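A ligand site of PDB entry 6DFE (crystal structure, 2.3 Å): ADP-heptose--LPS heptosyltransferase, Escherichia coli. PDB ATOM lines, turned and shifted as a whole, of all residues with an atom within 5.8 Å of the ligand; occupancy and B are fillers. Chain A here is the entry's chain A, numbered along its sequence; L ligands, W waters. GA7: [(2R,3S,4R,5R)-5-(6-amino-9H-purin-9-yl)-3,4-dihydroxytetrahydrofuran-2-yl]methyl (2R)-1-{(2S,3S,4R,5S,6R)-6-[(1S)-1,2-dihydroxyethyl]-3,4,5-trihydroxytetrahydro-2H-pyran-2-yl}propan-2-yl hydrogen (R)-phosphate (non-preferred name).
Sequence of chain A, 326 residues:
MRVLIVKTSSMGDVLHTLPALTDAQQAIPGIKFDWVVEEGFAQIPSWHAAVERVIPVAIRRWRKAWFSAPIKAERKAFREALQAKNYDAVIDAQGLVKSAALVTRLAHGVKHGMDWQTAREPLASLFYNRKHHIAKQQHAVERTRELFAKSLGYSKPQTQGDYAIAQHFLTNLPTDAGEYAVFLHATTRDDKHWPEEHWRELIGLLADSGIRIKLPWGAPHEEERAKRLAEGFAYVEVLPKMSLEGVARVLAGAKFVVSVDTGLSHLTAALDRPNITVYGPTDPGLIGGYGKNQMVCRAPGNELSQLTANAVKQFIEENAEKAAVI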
ATOM      1  N   MET A  11     -12.380  29.494  -5.075  1.00  0.00           N
ATOM      2  CA  MET A  11     -12.207  30.253  -3.854  1.00  0.00           C
ATOM      3  C   MET A  11     -10.823  30.880  -3.740  1.00  0.00           C
ATOM      4  O   MET A  11     -10.709  32.075  -3.452  1.00  0.00           O
ATOM      5  CB  MET A  11     -12.498  29.420  -2.602  1.00  0.00           C
ATOM      6  CG  MET A  11     -12.410  30.244  -1.301  1.00  0.00           C
ATOM      7  SD  MET A  11     -12.555  29.307   0.246  1.00  0.00           S
ATOM      8  CE  MET A  11     -14.226  28.683   0.093  1.00  0.00           C
ATOM      9  N   GLU A  38     -18.689  34.211  -8.502  1.00  0.00           N
ATOM     10  CA  GLU A  38     -19.702  33.141  -8.244  1.00  0.00           C
ATOM     11  C   GLU A  38     -20.383  33.396  -6.899  1.00  0.00           C
ATOM     12  O   GLU A  38     -19.762  33.831  -5.928  1.00  0.00           O
ATOM     13  CB  GLU A  38     -19.086  31.750  -8.208  1.00  0.00           C
ATOM     14  CG  GLU A  38     -18.944  31.066  -9.562  1.00  0.00           C
ATOM     15  CD  GLU A  38     -20.242  30.527 -10.138  1.00  0.00           C
ATOM     16  OE1 GLU A  38     -21.202  30.329  -9.365  1.00  0.00           O
ATOM     17  OE2 GLU A  38     -20.275  30.287 -11.377  1.00  0.00           O
ATOM     18  N   GLU A  39     -21.666  33.125  -6.858  1.00  0.00           N
ATOM     19  CA  GLU A  39     -22.462  33.401  -5.661  1.00  0.00           C
ATOM     20  C   GLU A  39     -21.877  32.810  -4.360  1.00  0.00           C
ATOM     21  O   GLU A  39     -21.916  33.447  -3.313  1.00  0.00           O
ATOM     22  CB  GLU A  39     -23.914  32.955  -5.888  1.00  0.00           C
ATOM     23  CG  GLU A  39     -24.079  31.455  -6.056  1.00  0.00           C
ATOM     24  CD  GLU A  39     -25.433  31.008  -6.613  1.00  0.00           C
ATOM     25  OE1 GLU A  39     -26.371  31.817  -6.800  1.00  0.00           O
ATOM     26  OE2 GLU A  39     -25.529  29.800  -6.848  1.00  0.00           O
ATOM     27  N   GLY A  40     -21.281  31.630  -4.439  1.00  0.00           N
ATOM     28  CA  GLY A  40     -20.711  30.992  -3.249  1.00  0.00           C
ATOM     29  C   GLY A  40     -19.559  31.748  -2.591  1.00  0.00           C
ATOM     30  O   GLY A  40     -19.309  31.566  -1.390  1.00  0.00           O
ATOM     31  N   PHE A  41     -18.882  32.600  -3.360  1.00  0.00           N
ATOM     32  CA  PHE A  41     -17.780  33.384  -2.903  1.00  0.00           C
ATOM     33  C   PHE A  41     -18.093  34.871  -2.815  1.00  0.00           C
ATOM     34  O   PHE A  41     -17.182  35.662  -2.589  1.00  0.00           O
ATOM     35  CB  PHE A  41     -16.555  33.178  -3.819  1.00  0.00           C
ATOM     36  CG  PHE A  41     -16.335  31.751  -4.236  1.00  0.00           C
ATOM     37  CD1 PHE A  41     -16.201  30.733  -3.283  1.00  0.00           C
ATOM     38  CD2 PHE A  41     -16.233  31.412  -5.579  1.00  0.00           C
ATOM     39  CE1 PHE A  41     -15.987  29.413  -3.657  1.00  0.00           C
ATOM     40  CE2 PHE A  41     -16.029  30.079  -5.967  1.00  0.00           C
ATOM     41  CZ  PHE A  41     -15.903  29.083  -5.008  1.00  0.00           C
ATOM     42  N   VAL A  57     -22.692  35.918  -9.993  1.00  0.00           N
ATOM     43  CA  VAL A  57     -23.090  35.037 -11.092  1.00  0.00           C
ATOM     44  C   VAL A  57     -23.251  33.669 -10.533  1.00  0.00           C
ATOM     45  O   VAL A  57     -22.676  33.343  -9.486  1.00  0.00           O
ATOM     46  CB  VAL A  57     -22.072  34.886 -12.249  1.00  0.00           C
ATOM     47  CG1 VAL A  57     -22.189  36.010 -13.208  1.00  0.00           C
ATOM     48  CG2 VAL A  57     -20.640  34.730 -11.786  1.00  0.00           C
ATOM     49  N   ALA A  58     -23.977  32.852 -11.301  1.00  0.00           N
ATOM     50  CA  ALA A  58     -24.138  31.461 -10.941  1.00  0.00           C
ATOM     51  C   ALA A  58     -23.989  30.564 -12.176  1.00  0.00           C
ATOM     52  O   ALA A  58     -24.791  29.685 -12.416  1.00  0.00           O
ATOM     53  CB  ALA A  58     -25.478  31.261 -10.245  1.00  0.00           C
ATOM     54  N   ARG A  60     -22.099  28.008 -12.813  1.00  0.00           N
ATOM     55  CA  ARG A  60     -22.044  26.558 -12.549  1.00  0.00           C
ATOM     56  C   ARG A  60     -23.436  25.967 -12.291  1.00  0.00           C
ATOM     57  O   ARG A  60     -23.752  24.881 -12.786  1.00  0.00           O
ATOM     58  CB  ARG A  60     -21.105  26.275 -11.367  1.00  0.00           C
ATOM     59  CG  ARG A  60     -19.659  26.579 -11.712  1.00  0.00           C
ATOM     60  CD  ARG A  60     -18.798  26.836 -10.482  1.00  0.00           C
ATOM     61  NE  ARG A  60     -17.390  26.590 -10.774  1.00  0.00           N
ATOM     62  CZ  ARG A  60     -16.412  26.555  -9.865  1.00  0.00           C
ATOM     63  NH1 ARG A  60     -16.645  26.806  -8.567  1.00  0.00           N
ATOM     64  NH2 ARG A  60     -15.176  26.287 -10.287  1.00  0.00           N
ATOM     65  N   ARG A  61     -24.263  26.708 -11.567  1.00  0.00           N
ATOM     66  CA  ARG A  61     -25.613  26.269 -11.271  1.00  0.00           C
ATOM     67  C   ARG A  61     -26.513  26.423 -12.489  1.00  0.00           C
ATOM     68  O   ARG A  61     -27.354  25.559 -12.755  1.00  0.00           O
ATOM     69  CB  ARG A  61     -26.149  27.072 -10.116  1.00  0.00           C
ATOM     70  CG  ARG A  61     -27.031  26.288  -9.170  1.00  0.00           C
ATOM     71  CD  ARG A  61     -27.644  27.229  -8.145  1.00  0.00           C
ATOM     72  NE  ARG A  61     -28.682  27.968  -8.846  1.00  0.00           N
ATOM     73  CZ  ARG A  61     -28.854  29.285  -8.885  1.00  0.00           C
ATOM     74  NH1 ARG A  61     -28.085  30.129  -8.213  1.00  0.00           N
ATOM     75  NH2 ARG A  61     -29.838  29.765  -9.618  1.00  0.00           N
ATOM     76  N   ALA A 186     -10.727  18.965   5.094  1.00  0.00           N
ATOM     77  CA  ALA A 186     -11.510  18.826   3.892  1.00  0.00           C
ATOM     78  C   ALA A 186     -10.839  19.415   2.632  1.00  0.00           C
ATOM     79  O   ALA A 186     -10.397  20.578   2.623  1.00  0.00           O
ATOM     80  CB  ALA A 186     -12.841  19.476   4.113  1.00  0.00           C
ATOM     81  N   THR A 187     -10.749  18.597   1.595  1.00  0.00           N
ATOM     82  CA  THR A 187     -10.252  19.024   0.293  1.00  0.00           C
ATOM     83  C   THR A 187     -10.997  18.268  -0.824  1.00  0.00           C
ATOM     84  O   THR A 187     -12.111  17.781  -0.622  1.00  0.00           O
ATOM     85  CB  THR A 187      -8.690  18.986   0.207  1.00  0.00           C
ATOM     86  OG1 THR A 187      -8.258  19.477  -1.064  1.00  0.00           O
ATOM     87  CG2 THR A 187      -8.081  17.607   0.436  1.00  0.00           C
ATOM     88  N   PRO A 216     -13.711  22.787  11.070  1.00  0.00           N
ATOM     89  CA  PRO A 216     -14.855  23.194  10.253  1.00  0.00           C
ATOM     90  C   PRO A 216     -15.286  22.133   9.252  1.00  0.00           C
ATOM     91  O   PRO A 216     -14.534  21.206   8.921  1.00  0.00           O
ATOM     92  CB  PRO A 216     -14.326  24.430   9.492  1.00  0.00           C
ATOM     93  CG  PRO A 216     -12.917  24.626   9.928  1.00  0.00           C
ATOM     94  CD  PRO A 216     -12.462  23.339  10.507  1.00  0.00           C
ATOM     95  N   TRP A 217     -16.490  22.345   8.729  1.00  0.00           N
ATOM     96  CA  TRP A 217     -17.023  21.482   7.705  1.00  0.00           C
ATOM     97  C   TRP A 217     -18.076  22.223   6.910  1.00  0.00           C
ATOM     98  O   TRP A 217     -18.755  23.087   7.458  1.00  0.00           O
ATOM     99  CB  TRP A 217     -17.609  20.211   8.341  1.00  0.00           C
ATOM    100  CG  TRP A 217     -18.727  20.503   9.341  1.00  0.00           C
ATOM    101  CD1 TRP A 217     -18.571  20.753  10.672  1.00  0.00           C
ATOM    102  CD2 TRP A 217     -20.132  20.553   9.077  1.00  0.00           C
ATOM    103  NE1 TRP A 217     -19.791  20.984  11.254  1.00  0.00           N
ATOM    104  CE2 TRP A 217     -20.772  20.850  10.300  1.00  0.00           C
ATOM    105  CE3 TRP A 217     -20.916  20.376   7.930  1.00  0.00           C
ATOM    106  CZ2 TRP A 217     -22.176  20.997  10.406  1.00  0.00           C
ATOM    107  CZ3 TRP A 217     -22.308  20.505   8.017  1.00  0.00           C
ATOM    108  CH2 TRP A 217     -22.925  20.799   9.267  1.00  0.00           C
ATOM    109  N   GLY A 218     -18.197  21.886   5.618  1.00  0.00           N
ATOM    110  CA  GLY A 218     -19.215  22.511   4.752  1.00  0.00           C
ATOM    111  C   GLY A 218     -20.061  21.588   3.921  1.00  0.00           C
ATOM    112  O   GLY A 218     -20.709  22.043   2.994  1.00  0.00           O
ATOM    113  N   ALA A 219     -20.022  20.299   4.215  1.00  0.00           N
ATOM    114  CA  ALA A 219     -20.880  19.301   3.562  1.00  0.00           C
ATOM    115  C   ALA A 219     -20.943  18.060   4.455  1.00  0.00           C
ATOM    116  O   ALA A 219     -20.008  17.813   5.205  1.00  0.00           O
ATOM    117  CB  ALA A 219     -20.363  18.950   2.163  1.00  0.00           C
ATOM    118  N   GLU A 222     -17.951  15.811   5.096  1.00  0.00           N
ATOM    119  CA  GLU A 222     -16.929  16.556   5.858  1.00  0.00           C
ATOM    120  C   GLU A 222     -17.242  16.624   7.366  1.00  0.00           C
ATOM    121  O   GLU A 222     -16.342  16.409   8.180  1.00  0.00           O
ATOM    122  CB  GLU A 222     -16.733  17.972   5.286  1.00  0.00           C
ATOM    123  CG  GLU A 222     -16.198  18.009   3.857  1.00  0.00           C
ATOM    124  CD  GLU A 222     -16.186  19.417   3.240  1.00  0.00           C
ATOM    125  OE1 GLU A 222     -16.515  20.419   3.929  1.00  0.00           O
ATOM    126  OE2 GLU A 222     -15.836  19.531   2.034  1.00  0.00           O
ATOM    127  N   MET A 242     -21.440  27.162   9.326  1.00  0.00           N
ATOM    128  CA  MET A 242     -21.494  28.633   9.283  1.00  0.00           C
ATOM    129  C   MET A 242     -21.298  29.134   7.879  1.00  0.00           C
ATOM    130  O   MET A 242     -20.995  28.357   6.965  1.00  0.00           O
ATOM    131  CB  MET A 242     -20.490  29.259  10.260  1.00  0.00           C
ATOM    132  CG  MET A 242     -19.185  28.485  10.465  1.00  0.00           C
ATOM    133  SD  MET A 242     -18.073  29.257  11.670  1.00  0.00           S
ATOM    134  CE  MET A 242     -19.165  29.900  12.943  1.00  0.00           C
ATOM    135  N   SER A 243     -21.483  30.439   7.718  1.00  0.00           N
ATOM    136  CA  SER A 243     -21.217  31.121   6.477  1.00  0.00           C
ATOM    137  C   SER A 243     -19.730  31.256   6.281  1.00  0.00           C
ATOM    138  O   SER A 243     -18.920  31.065   7.222  1.00  0.00           O
ATOM    139  CB  SER A 243     -21.792  32.515   6.505  1.00  0.00           C
ATOM    140  OG  SER A 243     -20.976  33.332   7.323  1.00  0.00           O
ATOM    141  N   LEU A 244     -19.374  31.610   5.053  1.00  0.00           N
ATOM    142  CA  LEU A 244     -17.980  31.795   4.716  1.00  0.00           C
ATOM    143  C   LEU A 244     -17.379  32.870   5.622  1.00  0.00           C
ATOM    144  O   LEU A 244     -16.257  32.717   6.117  1.00  0.00           O
ATOM    145  CB  LEU A 244     -17.815  32.158   3.234  1.00  0.00           C
ATOM    146  CG  LEU A 244     -16.441  32.037   2.565  1.00  0.00           C
ATOM    147  CD1 LEU A 244     -15.793  30.705   2.888  1.00  0.00           C
ATOM    148  CD2 LEU A 244     -16.596  32.179   1.057  1.00  0.00           C
ATOM    149  N   VAL A 247     -16.650  31.320   9.178  1.00  0.00           N
ATOM    150  CA  VAL A 247     -15.450  30.498   9.220  1.00  0.00           C
ATOM    151  C   VAL A 247     -14.202  31.374   9.076  1.00  0.00           C
ATOM    152  O   VAL A 247     -13.163  31.072   9.684  1.00  0.00           O
ATOM    153  CB  VAL A 247     -15.490  29.306   8.238  1.00  0.00           C
ATOM    154  CG1 VAL A 247     -15.504  29.764   6.787  1.00  0.00           C
ATOM    155  CG2 VAL A 247     -14.261  28.433   8.429  1.00  0.00           C
ATOM    156  N   THR A 262      -6.317  23.305  -0.003  1.00  0.00           N
ATOM    157  CA  THR A 262      -7.761  23.473  -0.044  1.00  0.00           C
ATOM    158  C   THR A 262      -8.062  24.976   0.014  1.00  0.00           C
ATOM    159  O   THR A 262      -7.238  25.776   0.446  1.00  0.00           O
ATOM    160  CB  THR A 262      -8.454  22.693   1.129  1.00  0.00           C
ATOM    161  OG1 THR A 262      -9.887  22.617   0.944  1.00  0.00           O
ATOM    162  CG2 THR A 262      -8.155  23.360   2.507  1.00  0.00           C
ATOM    163  N   GLY A 263      -9.263  25.321  -0.432  1.00  0.00           N
ATOM    164  CA  GLY A 263      -9.736  26.669  -0.450  1.00  0.00           C
ATOM    165  C   GLY A 263      -9.502  27.439   0.826  1.00  0.00           C
ATOM    166  O   GLY A 263      -9.001  28.564   0.802  1.00  0.00           O
ATOM    167  N   LEU A 264      -9.859  26.824   1.963  1.00  0.00           N
ATOM    168  CA  LEU A 264      -9.834  27.517   3.236  1.00  0.00           C
ATOM    169  C   LEU A 264      -8.396  27.714   3.739  1.00  0.00           C
ATOM    170  O   LEU A 264      -8.175  28.589   4.575  1.00  0.00           O
ATOM    171  CB  LEU A 264     -10.671  26.770   4.266  1.00  0.00           C
ATOM    172  CG  LEU A 264     -12.204  26.760   4.120  1.00  0.00           C
ATOM    173  CD1 LEU A 264     -12.800  25.848   5.200  1.00  0.00           C
ATOM    174  CD2 LEU A 264     -12.728  28.185   4.178  1.00  0.00           C
HETATM  175  O7  GA7 L   1     -16.542  26.244  -3.629  1.00  0.00           O
HETATM  176  P   GA7 L   1     -17.223  25.388  -2.586  1.00  0.00           P
HETATM  177  O6  GA7 L   1     -17.498  24.011  -3.142  1.00  0.00           O
HETATM  178  O4  GA7 L   1     -18.722  25.871  -2.147  1.00  0.00           O
HETATM  179  C7  GA7 L   1     -19.306  27.185  -2.103  1.00  0.00           C
HETATM  180  C8  GA7 L   1     -18.697  28.028  -0.986  1.00  0.00           C
HETATM  181  C4  GA7 L   1     -20.836  27.094  -1.909  1.00  0.00           C
HETATM  182  C   GA7 L   1     -21.619  26.760  -3.202  1.00  0.00           C
HETATM  183  C5  GA7 L   1     -23.143  26.881  -3.109  1.00  0.00           C
HETATM  184  O3  GA7 L   1     -23.430  28.180  -2.568  1.00  0.00           O
HETATM  185  C6  GA7 L   1     -23.873  26.722  -4.482  1.00  0.00           C
HETATM  186  O2  GA7 L   1     -25.232  27.246  -4.442  1.00  0.00           O
HETATM  187  C1  GA7 L   1     -23.124  27.409  -5.653  1.00  0.00           C
HETATM  188  O1  GA7 L   1     -23.509  26.855  -6.934  1.00  0.00           O
HETATM  189  C2  GA7 L   1     -21.592  27.354  -5.553  1.00  0.00           C
HETATM  190  C3  GA7 L   1     -20.873  28.307  -6.538  1.00  0.00           C
HETATM  191  O12 GA7 L   1     -21.215  29.704  -6.403  1.00  0.00           O
HETATM  192  C19 GA7 L   1     -19.377  28.218  -6.373  1.00  0.00           C
HETATM  193  O11 GA7 L   1     -18.999  27.048  -7.056  1.00  0.00           O
HETATM  194  O   GA7 L   1     -21.200  27.683  -4.203  1.00  0.00           O
HETATM  195  O5  GA7 L   1     -16.170  25.286  -1.362  1.00  0.00           O
HETATM  196  C18 GA7 L   1     -14.848  24.720  -1.510  1.00  0.00           C
HETATM  197  C17 GA7 L   1     -14.355  23.943  -0.255  1.00  0.00           C
HETATM  198  C14 GA7 L   1     -15.194  22.731   0.162  1.00  0.00           C
HETATM  199  O10 GA7 L   1     -14.339  21.724   0.759  1.00  0.00           O
HETATM  200  C15 GA7 L   1     -16.134  23.290   1.203  1.00  0.00           C
HETATM  201  O9  GA7 L   1     -16.633  22.333   2.128  1.00  0.00           O
HETATM  202  C16 GA7 L   1     -15.268  24.345   1.901  1.00  0.00           C
HETATM  203  O8  GA7 L   1     -14.338  24.798   0.904  1.00  0.00           O
HETATM  204  N2  GA7 L   1     -16.164  25.403   2.437  1.00  0.00           N
HETATM  205  C10 GA7 L   1     -16.503  25.515   3.732  1.00  0.00           C
HETATM  206  N1  GA7 L   1     -16.176  24.839   4.893  1.00  0.00           N
HETATM  207  C9  GA7 L   1     -16.719  25.234   6.080  1.00  0.00           C
HETATM  208  N   GA7 L   1     -17.580  26.261   6.215  1.00  0.00           N
HETATM  209  C12 GA7 L   1     -17.982  27.016   5.126  1.00  0.00           C
HETATM  210  N4  GA7 L   1     -18.844  28.075   5.241  1.00  0.00           N
HETATM  211  C11 GA7 L   1     -17.439  26.663   3.785  1.00  0.00           C
HETATM  212  N3  GA7 L   1     -17.573  27.133   2.526  1.00  0.00           N
HETATM  213  C13 GA7 L   1     -16.812  26.359   1.722  1.00  0.00           C
HETATM  214  O   HOH W   1     -11.605  24.353   1.671  1.00  0.00           O
HETATM  215  O   HOH W   2     -23.215  28.487  -9.108  1.00  0.00           O
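O9 of the ligand lies within hydrogen-bond range of OE1 of Glu 222.
The backbone NH of Gly 40 sits at hydrogen-bond distance from an oxygen (O12) of the ligand, 2.8 Å away.
O of Met 242 lies within hydrogen-bond range of N4 of the ligand (2.8 Å).
O11 of the ligand sits at hydrogen-bond distance from NH1 of Arg 60.
The side-chain carboxylate (OE1) of Glu 38 lies within hydrogen-bond range of an oxygen (O12) of the ligand, 3.0 Å away.
The backbone NH of Glu 39 sits close to an oxygen (O12) of the ligand (3.5 Å).
The backbone NH (N) of Gly 218 is in hydrogen-bond range of the side-chain carboxylate (OE1) of Glu 222, 2.8 Å away.
The side-chain sulfur (SD) of Met 242 sits at hydrogen-bond distance from the backbone NH (N) of Val 247, at 3.5 Å.
The backbone NH (N) of Arg 60 is in hydrogen-bond range of the side-chain carboxylate (OE2) of Glu 38, 3.3 Å away.
OE1 of Glu 39 is in salt-bridge range of NH1 of Arg 61, 2.8 Å away.
N of Glu 39 sits at hydrogen-bond distance from O of Val 57, 2.8 Å away.
CE of Met 11 touches C13 of the ligand, 3.8 Å away.
Phe 41 touches the ligand.
Trp 217 touches the ligand.
N of Gly 218 touches N1 of the ligand (3.7 Å).
Ser 243 touches the ligand.
Leu 244 touches the ligand.
CD1 of Leu 264 touches N1 of the ligand, at 3.5 Å.
Hydrophobic or aromatic side chains that line the ligand: Met 11, Phe 41 and Leu 264.
Water W2 lies within hydrogen-bond range of O1 of the ligand, OE1 of Glu 38, N of Arg 61 and OE2 of Glu 39.
Water W1 lies within hydrogen-bond range of the side-chain hydroxyl (OG1) of Thr 262, an oxygen (O8) of the ligand, the backbone NH (N) of Leu 264 and the backbone NH (N) of Gly 263.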
